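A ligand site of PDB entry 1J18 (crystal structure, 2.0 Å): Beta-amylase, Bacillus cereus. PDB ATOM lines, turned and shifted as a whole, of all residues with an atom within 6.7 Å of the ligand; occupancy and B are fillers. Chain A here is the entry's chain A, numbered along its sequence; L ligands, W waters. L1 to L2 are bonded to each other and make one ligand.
O2 of LIG L1 sits at hydrogen-bond distance from OE1 of Gln 239 (2.6 Å). The backbone carbonyl oxygen (O) of Ala 230 lies within hydrogen-bond range of an oxygen (O3) of LG2 L2 (2.6 Å). The backbone NH (N) of Leu 232 lies within hydrogen-bond range of an oxygen (O5) of LG2 L2, at 2.7 Å. O of Leu 232 is in hydrogen-bond range of O5 of LG2 L2 (3.0 Å). N of Ser 235 sits at hydrogen-bond distance from O1 of LG2 L2 (2.8 Å). O1 of LG2 L2 lies within hydrogen-bond range of OG of Ser 235 (2.9 Å). The side-chain hydroxyl (OH) of Tyr 249 sits close to an oxygen (O4) of LG2 L2, 3.4 Å away.
Water W4 lies within hydrogen-bond range of O3 of LIG L1 (2.6 Å), N of Asp 236 (2.9 Å), OE1 of Gln 239 (3.0 Å) and N of Ser 235 (3.4 Å). Water W3 lies within hydrogen-bond range of an oxygen (O1) of LG2 L2 (2.7 Å) and the side-chain hydroxyl of Ser 235 (3.0 Å). Water W1 lies within hydrogen-bond range of an oxygen (O5) of LIG L1 (3.0 Å) and the side-chain hydroxyl (OG) of Ser 247 (3.4 Å).
CZ3 of Trp 221 touches O5 of LG2 L2, 3.7 Å away. CG2 of Thr 223 touches O6 of LIG L1 (3.5 Å). CD2 of Leu 225 touches O3 of LG2 L2 (3.7 Å). CA of Ile 231 touches O5 of LG2 L2, at 3.3 Å. O of Pro 233 touches C2 of LG2 L2, at 3.5 Å. CA of Pro 234 touches O3 of LIG L1 (3.4 Å). CA of Phe 240 touches O2 of LIG L1 (3.4 Å). Gly 244 touches the ligand. OG of Ser 247 touches O1 of LIG L1 (3.8 Å). Hydrophobic or aromatic side chains that line the ligand: Trp 221, Leu 225, Leu 232, Pro 234, Phe 240 and Tyr 249. Within 4 Å of the ligand: Trp 221, Thr 223, Leu 225, Ala 230, Ile 231, Leu 232, Pro 233, Pro 234, Ser 235, Gln 239, Phe 240, Gly 244, Ser 247 and Tyr 249.
N of Gly 244 sits at hydrogen-bond distance from O of Gln 239 (3.2 Å). OD1 of Asp 236 lies within hydrogen-bond range of N of Gln 239, at 3.1 Å. The side-chain amide nitrogen (NE2) of Gln 239 sits close to the side-chain amide nitrogen (ND2) of Asn 243. The backbone carbonyl oxygen (O) of Leu 232 lies within hydrogen-bond range of the side-chain hydroxyl (OH) of Tyr 249 (2.7 Å). The backbone carbonyl oxygen (O) of Gly 244 is in hydrogen-bond range of the side-chain hydroxyl (OG) of Ser 247 (2.8 Å). The backbone NH of Tyr 249 sits close to the side-chain hydroxyl of Ser 247 (3.5 Å). O of Phe 240 lies within hydrogen-bond range of N of Tyr 245 (2.8 Å). The side-chain hydroxyl of Ser 247 is in hydrogen-bond range of the backbone NH of Gly 250, 3.1 Å away.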
ATOM      1  N   PHE A 203      -5.756 -22.857 -28.383  1.00  0.00           N
ATOM      2  CA  PHE A 203      -6.213 -21.729 -27.602  1.00  0.00           C
ATOM      3  C   PHE A 203      -5.277 -20.549 -27.811  1.00  0.00           C
ATOM      4  O   PHE A 203      -5.719 -19.410 -28.019  1.00  0.00           O
ATOM      5  CB  PHE A 203      -6.278 -22.079 -26.109  1.00  0.00           C
ATOM      6  CG  PHE A 203      -6.682 -20.916 -25.238  1.00  0.00           C
ATOM      7  CD1 PHE A 203      -7.850 -20.215 -25.490  1.00  0.00           C
ATOM      8  CD2 PHE A 203      -5.887 -20.538 -24.153  1.00  0.00           C
ATOM      9  CE1 PHE A 203      -8.228 -19.126 -24.686  1.00  0.00           C
ATOM     10  CE2 PHE A 203      -6.257 -19.455 -23.344  1.00  0.00           C
ATOM     11  CZ  PHE A 203      -7.429 -18.753 -23.614  1.00  0.00           C
ATOM     12  N   TRP A 221      -6.284  -8.412 -21.371  1.00  0.00           N
ATOM     13  CA  TRP A 221      -6.482  -9.170 -20.134  1.00  0.00           C
ATOM     14  C   TRP A 221      -5.933  -8.485 -18.902  1.00  0.00           C
ATOM     15  O   TRP A 221      -6.229  -8.917 -17.786  1.00  0.00           O
ATOM     16  CB  TRP A 221      -5.843 -10.556 -20.245  1.00  0.00           C
ATOM     17  CG  TRP A 221      -6.457 -11.457 -21.267  1.00  0.00           C
ATOM     18  CD1 TRP A 221      -7.619 -11.259 -21.950  1.00  0.00           C
ATOM     19  CD2 TRP A 221      -5.916 -12.701 -21.719  1.00  0.00           C
ATOM     20  NE1 TRP A 221      -7.845 -12.315 -22.803  1.00  0.00           N
ATOM     21  CE2 TRP A 221      -6.819 -13.212 -22.678  1.00  0.00           C
ATOM     22  CE3 TRP A 221      -4.762 -13.437 -21.411  1.00  0.00           C
ATOM     23  CZ2 TRP A 221      -6.603 -14.434 -23.333  1.00  0.00           C
ATOM     24  CZ3 TRP A 221      -4.558 -14.649 -22.058  1.00  0.00           C
ATOM     25  CH2 TRP A 221      -5.469 -15.126 -23.008  1.00  0.00           C
ATOM     26  N   GLY A 222      -5.131  -7.451 -19.097  1.00  0.00           N
ATOM     27  CA  GLY A 222      -4.545  -6.755 -17.968  1.00  0.00           C
ATOM     28  C   GLY A 222      -3.478  -7.621 -17.331  1.00  0.00           C
ATOM     29  O   GLY A 222      -3.221  -7.551 -16.139  1.00  0.00           O
ATOM     30  N   THR A 223      -2.850  -8.455 -18.154  1.00  0.00           N
ATOM     31  CA  THR A 223      -1.819  -9.363 -17.694  1.00  0.00           C
ATOM     32  C   THR A 223      -0.416  -8.882 -18.063  1.00  0.00           C
ATOM     33  O   THR A 223      -0.256  -7.862 -18.725  1.00  0.00           O
ATOM     34  CB  THR A 223      -2.055 -10.765 -18.263  1.00  0.00           C
ATOM     35  OG1 THR A 223      -2.154 -10.685 -19.698  1.00  0.00           O
ATOM     36  CG2 THR A 223      -3.352 -11.345 -17.706  1.00  0.00           C
ATOM     37  N   LEU A 225       2.046 -11.297 -19.317  1.00  0.00           N
ATOM     38  CA  LEU A 225       2.630 -12.514 -19.860  1.00  0.00           C
ATOM     39  C   LEU A 225       3.938 -12.147 -20.530  1.00  0.00           C
ATOM     40  O   LEU A 225       4.029 -11.164 -21.255  1.00  0.00           O
ATOM     41  CB  LEU A 225       1.664 -13.137 -20.867  1.00  0.00           C
ATOM     42  CG  LEU A 225       0.253 -13.409 -20.327  1.00  0.00           C
ATOM     43  CD1 LEU A 225      -0.587 -14.066 -21.409  1.00  0.00           C
ATOM     44  CD2 LEU A 225       0.336 -14.300 -19.088  1.00  0.00           C
ATOM     45  N   LEU A 229       3.937 -18.382 -25.097  1.00  0.00           N
ATOM     46  CA  LEU A 229       3.830 -19.684 -24.446  1.00  0.00           C
ATOM     47  C   LEU A 229       3.166 -19.586 -23.076  1.00  0.00           C
ATOM     48  O   LEU A 229       2.769 -20.599 -22.505  1.00  0.00           O
ATOM     49  CB  LEU A 229       5.208 -20.333 -24.337  1.00  0.00           C
ATOM     50  CG  LEU A 229       5.870 -20.703 -25.676  1.00  0.00           C
ATOM     51  CD1 LEU A 229       7.320 -21.060 -25.458  1.00  0.00           C
ATOM     52  CD2 LEU A 229       5.118 -21.858 -26.332  1.00  0.00           C
ATOM     53  N   ALA A 230       3.045 -18.375 -22.553  1.00  0.00           N
ATOM     54  CA  ALA A 230       2.408 -18.166 -21.264  1.00  0.00           C
ATOM     55  C   ALA A 230       0.891 -18.116 -21.426  1.00  0.00           C
ATOM     56  O   ALA A 230       0.158 -18.128 -20.446  1.00  0.00           O
ATOM     57  CB  ALA A 230       2.913 -16.878 -20.624  1.00  0.00           C
ATOM     58  N   ILE A 231       0.429 -18.047 -22.679  1.00  0.00           N
ATOM     59  CA  ILE A 231      -1.022 -18.045 -22.945  1.00  0.00           C
ATOM     60  C   ILE A 231      -1.438 -19.503 -22.787  1.00  0.00           C
ATOM     61  O   ILE A 231      -1.089 -20.340 -23.615  1.00  0.00           O
ATOM     62  CB  ILE A 231      -1.339 -17.585 -24.385  1.00  0.00           C
ATOM     63  CG1 ILE A 231      -0.963 -16.109 -24.570  1.00  0.00           C
ATOM     64  CG2 ILE A 231      -2.833 -17.774 -24.664  1.00  0.00           C
ATOM     65  CD1 ILE A 231      -1.091 -15.605 -26.008  1.00  0.00           C
ATOM     66  N   LEU A 232      -2.170 -19.798 -21.723  1.00  0.00           N
ATOM     67  CA  LEU A 232      -2.578 -21.166 -21.447  1.00  0.00           C
ATOM     68  C   LEU A 232      -3.972 -21.262 -20.842  1.00  0.00           C
ATOM     69  O   LEU A 232      -4.522 -20.269 -20.369  1.00  0.00           O
ATOM     70  CB  LEU A 232      -1.591 -21.795 -20.452  1.00  0.00           C
ATOM     71  CG  LEU A 232      -0.119 -21.851 -20.835  1.00  0.00           C
ATOM     72  CD1 LEU A 232       0.734 -21.994 -19.584  1.00  0.00           C
ATOM     73  CD2 LEU A 232       0.100 -23.018 -21.785  1.00  0.00           C
ATOM     74  N   PRO A 233      -4.549 -22.478 -20.840  1.00  0.00           N
ATOM     75  CA  PRO A 233      -5.880 -22.686 -20.244  1.00  0.00           C
ATOM     76  C   PRO A 233      -5.626 -22.527 -18.748  1.00  0.00           C
ATOM     77  O   PRO A 233      -4.475 -22.450 -18.329  1.00  0.00           O
ATOM     78  CB  PRO A 233      -6.206 -24.128 -20.630  1.00  0.00           C
ATOM     79  CG  PRO A 233      -5.450 -24.329 -21.909  1.00  0.00           C
ATOM     80  CD  PRO A 233      -4.129 -23.670 -21.584  1.00  0.00           C
ATOM     81  N   PRO A 234      -6.686 -22.499 -17.922  1.00  0.00           N
ATOM     82  CA  PRO A 234      -6.508 -22.351 -16.469  1.00  0.00           C
ATOM     83  C   PRO A 234      -5.566 -23.381 -15.833  1.00  0.00           C
ATOM     84  O   PRO A 234      -5.692 -24.577 -16.061  1.00  0.00           O
ATOM     85  CB  PRO A 234      -7.929 -22.474 -15.941  1.00  0.00           C
ATOM     86  CG  PRO A 234      -8.779 -21.972 -17.097  1.00  0.00           C
ATOM     87  CD  PRO A 234      -8.112 -22.624 -18.267  1.00  0.00           C
ATOM     88  N   SER A 235      -4.607 -22.891 -15.046  1.00  0.00           N
ATOM     89  CA  SER A 235      -3.667 -23.781 -14.377  1.00  0.00           C
ATOM     90  C   SER A 235      -4.277 -24.288 -13.079  1.00  0.00           C
ATOM     91  O   SER A 235      -3.896 -25.337 -12.561  1.00  0.00           O
ATOM     92  CB  SER A 235      -2.354 -23.047 -14.067  1.00  0.00           C
ATOM     93  OG  SER A 235      -2.522 -22.158 -12.974  1.00  0.00           O
ATOM     94  N   ASP A 236      -5.236 -23.539 -12.554  1.00  0.00           N
ATOM     95  CA  ASP A 236      -5.927 -23.904 -11.318  1.00  0.00           C
ATOM     96  C   ASP A 236      -7.425 -23.874 -11.585  1.00  0.00           C
ATOM     97  O   ASP A 236      -8.063 -22.822 -11.429  1.00  0.00           O
ATOM     98  CB  ASP A 236      -5.575 -22.933 -10.198  1.00  0.00           C
ATOM     99  CG  ASP A 236      -6.077 -23.389  -8.838  1.00  0.00           C
ATOM    100  OD1 ASP A 236      -7.120 -24.082  -8.797  1.00  0.00           O
ATOM    101  OD2 ASP A 236      -5.453 -23.041  -7.818  1.00  0.00           O
ATOM    102  N   GLY A 237      -7.975 -25.014 -11.988  1.00  0.00           N
ATOM    103  CA  GLY A 237      -9.396 -25.103 -12.298  1.00  0.00           C
ATOM    104  C   GLY A 237     -10.312 -24.577 -11.220  1.00  0.00           C
ATOM    105  O   GLY A 237     -11.313 -23.919 -11.515  1.00  0.00           O
ATOM    106  N   GLN A 239      -9.641 -22.308  -8.736  1.00  0.00           N
ATOM    107  CA  GLN A 239      -9.555 -20.860  -8.654  1.00  0.00           C
ATOM    108  C   GLN A 239     -10.268 -20.224  -9.842  1.00  0.00           C
ATOM    109  O   GLN A 239     -10.924 -19.186  -9.694  1.00  0.00           O
ATOM    110  CB  GLN A 239      -8.078 -20.439  -8.609  1.00  0.00           C
ATOM    111  CG  GLN A 239      -7.822 -18.929  -8.561  1.00  0.00           C
ATOM    112  CD  GLN A 239      -7.766 -18.297  -9.935  1.00  0.00           C
ATOM    113  OE1 GLN A 239      -7.223 -18.869 -10.882  1.00  0.00           O
ATOM    114  NE2 GLN A 239      -8.318 -17.089 -10.053  1.00  0.00           N
ATOM    115  N   PHE A 240     -10.159 -20.838 -11.016  1.00  0.00           N
ATOM    116  CA  PHE A 240     -10.828 -20.279 -12.186  1.00  0.00           C
ATOM    117  C   PHE A 240     -12.336 -20.219 -11.972  1.00  0.00           C
ATOM    118  O   PHE A 240     -12.984 -19.222 -12.270  1.00  0.00           O
ATOM    119  CB  PHE A 240     -10.539 -21.103 -13.438  1.00  0.00           C
ATOM    120  CG  PHE A 240     -11.148 -20.519 -14.685  1.00  0.00           C
ATOM    121  CD1 PHE A 240     -10.517 -19.474 -15.345  1.00  0.00           C
ATOM    122  CD2 PHE A 240     -12.378 -20.973 -15.160  1.00  0.00           C
ATOM    123  CE1 PHE A 240     -11.104 -18.871 -16.466  1.00  0.00           C
ATOM    124  CE2 PHE A 240     -12.980 -20.385 -16.272  1.00  0.00           C
ATOM    125  CZ  PHE A 240     -12.333 -19.334 -16.930  1.00  0.00           C
ATOM    126  N   LEU A 241     -12.883 -21.323 -11.461  1.00  0.00           N
ATOM    127  CA  LEU A 241     -14.320 -21.429 -11.218  1.00  0.00           C
ATOM    128  C   LEU A 241     -14.798 -20.555 -10.067  1.00  0.00           C
ATOM    129  O   LEU A 241     -15.966 -20.193  -9.995  1.00  0.00           O
ATOM    130  CB  LEU A 241     -14.691 -22.889 -10.952  1.00  0.00           C
ATOM    131  CG  LEU A 241     -14.531 -23.798 -12.173  1.00  0.00           C
ATOM    132  CD1 LEU A 241     -14.671 -25.263 -11.778  1.00  0.00           C
ATOM    133  CD2 LEU A 241     -15.575 -23.409 -13.213  1.00  0.00           C
ATOM    134  N   ASN A 243     -13.307 -17.434  -9.172  1.00  0.00           N
ATOM    135  CA  ASN A 243     -13.286 -16.031  -9.573  1.00  0.00           C
ATOM    136  C   ASN A 243     -12.610 -15.731 -10.907  1.00  0.00           C
ATOM    137  O   ASN A 243     -12.824 -14.656 -11.478  1.00  0.00           O
ATOM    138  CB  ASN A 243     -12.609 -15.196  -8.483  1.00  0.00           C
ATOM    139  CG  ASN A 243     -11.219 -15.696  -8.143  1.00  0.00           C
ATOM    140  OD1 ASN A 243     -11.062 -16.584  -7.315  1.00  0.00           O
ATOM    141  ND2 ASN A 243     -10.214 -15.130  -8.792  1.00  0.00           N
ATOM    142  N   GLY A 244     -11.793 -16.646 -11.406  1.00  0.00           N
ATOM    143  CA  GLY A 244     -11.118 -16.407 -12.670  1.00  0.00           C
ATOM    144  C   GLY A 244     -12.045 -16.170 -13.845  1.00  0.00           C
ATOM    145  O   GLY A 244     -11.755 -15.373 -14.746  1.00  0.00           O
ATOM    146  N   TYR A 245     -13.183 -16.859 -13.843  1.00  0.00           N
ATOM    147  CA  TYR A 245     -14.146 -16.745 -14.936  1.00  0.00           C
ATOM    148  C   TYR A 245     -14.670 -15.332 -15.162  1.00  0.00           C
ATOM    149  O   TYR A 245     -15.169 -15.013 -16.237  1.00  0.00           O
ATOM    150  CB  TYR A 245     -15.336 -17.693 -14.704  1.00  0.00           C
ATOM    151  CG  TYR A 245     -16.253 -17.274 -13.564  1.00  0.00           C
ATOM    152  CD1 TYR A 245     -15.921 -17.556 -12.241  1.00  0.00           C
ATOM    153  CD2 TYR A 245     -17.443 -16.611 -13.824  1.00  0.00           C
ATOM    154  CE1 TYR A 245     -16.769 -17.176 -11.198  1.00  0.00           C
ATOM    155  CE2 TYR A 245     -18.298 -16.226 -12.786  1.00  0.00           C
ATOM    156  CZ  TYR A 245     -17.949 -16.514 -11.478  1.00  0.00           C
ATOM    157  OH  TYR A 245     -18.777 -16.133 -10.446  1.00  0.00           O
ATOM    158  N   LEU A 246     -14.553 -14.491 -14.137  1.00  0.00           N
ATOM    159  CA  LEU A 246     -15.050 -13.113 -14.216  1.00  0.00           C
ATOM    160  C   LEU A 246     -14.155 -12.183 -15.035  1.00  0.00           C
ATOM    161  O   LEU A 246     -14.628 -11.184 -15.570  1.00  0.00           O
ATOM    162  CB  LEU A 246     -15.225 -12.542 -12.810  1.00  0.00           C
ATOM    163  CG  LEU A 246     -16.275 -13.248 -11.942  1.00  0.00           C
ATOM    164  CD1 LEU A 246     -16.100 -12.865 -10.484  1.00  0.00           C
ATOM    165  CD2 LEU A 246     -17.668 -12.885 -12.443  1.00  0.00           C
ATOM    166  N   SER A 247     -12.871 -12.512 -15.130  1.00  0.00           N
ATOM    167  CA  SER A 247     -11.925 -11.679 -15.850  1.00  0.00           C
ATOM    168  C   SER A 247     -12.107 -11.753 -17.371  1.00  0.00           C
ATOM    169  O   SER A 247     -12.800 -12.631 -17.892  1.00  0.00           O
ATOM    170  CB  SER A 247     -10.495 -12.082 -15.487  1.00  0.00           C
ATOM    171  OG  SER A 247     -10.180 -13.373 -15.976  1.00  0.00           O
ATOM    172  N   TYR A 249      -9.896 -12.529 -19.323  1.00  0.00           N
ATOM    173  CA  TYR A 249      -9.228 -13.761 -19.702  1.00  0.00           C
ATOM    174  C   TYR A 249     -10.250 -14.894 -19.616  1.00  0.00           C
ATOM    175  O   TYR A 249     -10.399 -15.689 -20.551  1.00  0.00           O
ATOM    176  CB  TYR A 249      -8.058 -14.074 -18.769  1.00  0.00           C
ATOM    177  CG  TYR A 249      -7.663 -15.541 -18.806  1.00  0.00           C
ATOM    178  CD1 TYR A 249      -6.933 -16.041 -19.879  1.00  0.00           C
ATOM    179  CD2 TYR A 249      -8.091 -16.426 -17.813  1.00  0.00           C
ATOM    180  CE1 TYR A 249      -6.638 -17.405 -19.970  1.00  0.00           C
ATOM    181  CE2 TYR A 249      -7.794 -17.782 -17.898  1.00  0.00           C
ATOM    182  CZ  TYR A 249      -7.076 -18.264 -18.974  1.00  0.00           C
ATOM    183  OH  TYR A 249      -6.793 -19.610 -19.067  1.00  0.00           O
ATOM    184  N   GLY A 250     -10.936 -14.963 -18.481  1.00  0.00           N
ATOM    185  CA  GLY A 250     -11.923 -15.997 -18.264  1.00  0.00           C
ATOM    186  C   GLY A 250     -13.012 -16.005 -19.327  1.00  0.00           C
ATOM    187  O   GLY A 250     -13.390 -17.066 -19.824  1.00  0.00           O
HETATM  188  C1  LIG L   1      -7.653 -17.295 -13.975  1.00  0.00           C
HETATM  189  C2  LIG L   1      -6.384 -18.036 -14.353  1.00  0.00           C
HETATM  190  C3  LIG L   1      -5.554 -17.206 -15.343  1.00  0.00           C
HETATM  191  C4  LIG L   1      -5.321 -15.787 -14.796  1.00  0.00           C
HETATM  192  C5  LIG L   1      -4.667 -14.883 -15.837  1.00  0.00           C
HETATM  193  C6  LIG L   1      -7.288 -15.906 -13.439  1.00  0.00           C
HETATM  194  O1  LIG L   1      -8.436 -15.211 -13.118  1.00  0.00           O
HETATM  195  O2  LIG L   1      -8.371 -18.033 -13.001  1.00  0.00           O
HETATM  196  O3  LIG L   1      -6.698 -19.292 -14.938  1.00  0.00           O
HETATM  197  O4  LIG L   1      -4.299 -17.845 -15.574  1.00  0.00           O
HETATM  198  O5  LIG L   1      -6.583 -15.170 -14.441  1.00  0.00           O
HETATM  199  O6  LIG L   1      -4.327 -13.623 -15.269  1.00  0.00           O
HETATM  200  C1  LG2 L   2      -4.280 -18.718 -16.664  1.00  0.00           C
HETATM  201  C2  LG2 L   2      -3.227 -19.803 -16.460  1.00  0.00           C
HETATM  202  C3  LG2 L   2      -1.817 -19.181 -16.550  1.00  0.00           C
HETATM  203  C4  LG2 L   2      -1.669 -18.433 -17.876  1.00  0.00           C
HETATM  204  C5  LG2 L   2      -2.787 -17.388 -18.014  1.00  0.00           C
HETATM  205  C6  LG2 L   2      -2.775 -16.729 -19.373  1.00  0.00           C
HETATM  206  O1  LG2 L   2      -3.402 -20.412 -15.179  1.00  0.00           O
HETATM  207  O2  LG2 L   2      -0.838 -20.200 -16.465  1.00  0.00           O
HETATM  208  O3  LG2 L   2      -0.401 -17.787 -17.924  1.00  0.00           O
HETATM  209  O4  LG2 L   2      -4.069 -18.031 -17.893  1.00  0.00           O
HETATM  210  O5  LG2 L   2      -3.126 -17.649 -20.385  1.00  0.00           O
HETATM  211  O   HOH W   1      -7.099 -12.291 -15.134  1.00  0.00           O
HETATM  212  O   HOH W   2       0.454 -16.056 -15.732  1.00  0.00           O
HETATM  213  O   HOH W   3      -3.651 -19.360 -12.726  1.00  0.00           O
HETATM  214  O   HOH W   4      -6.249 -20.856 -12.887  1.00  0.00           O
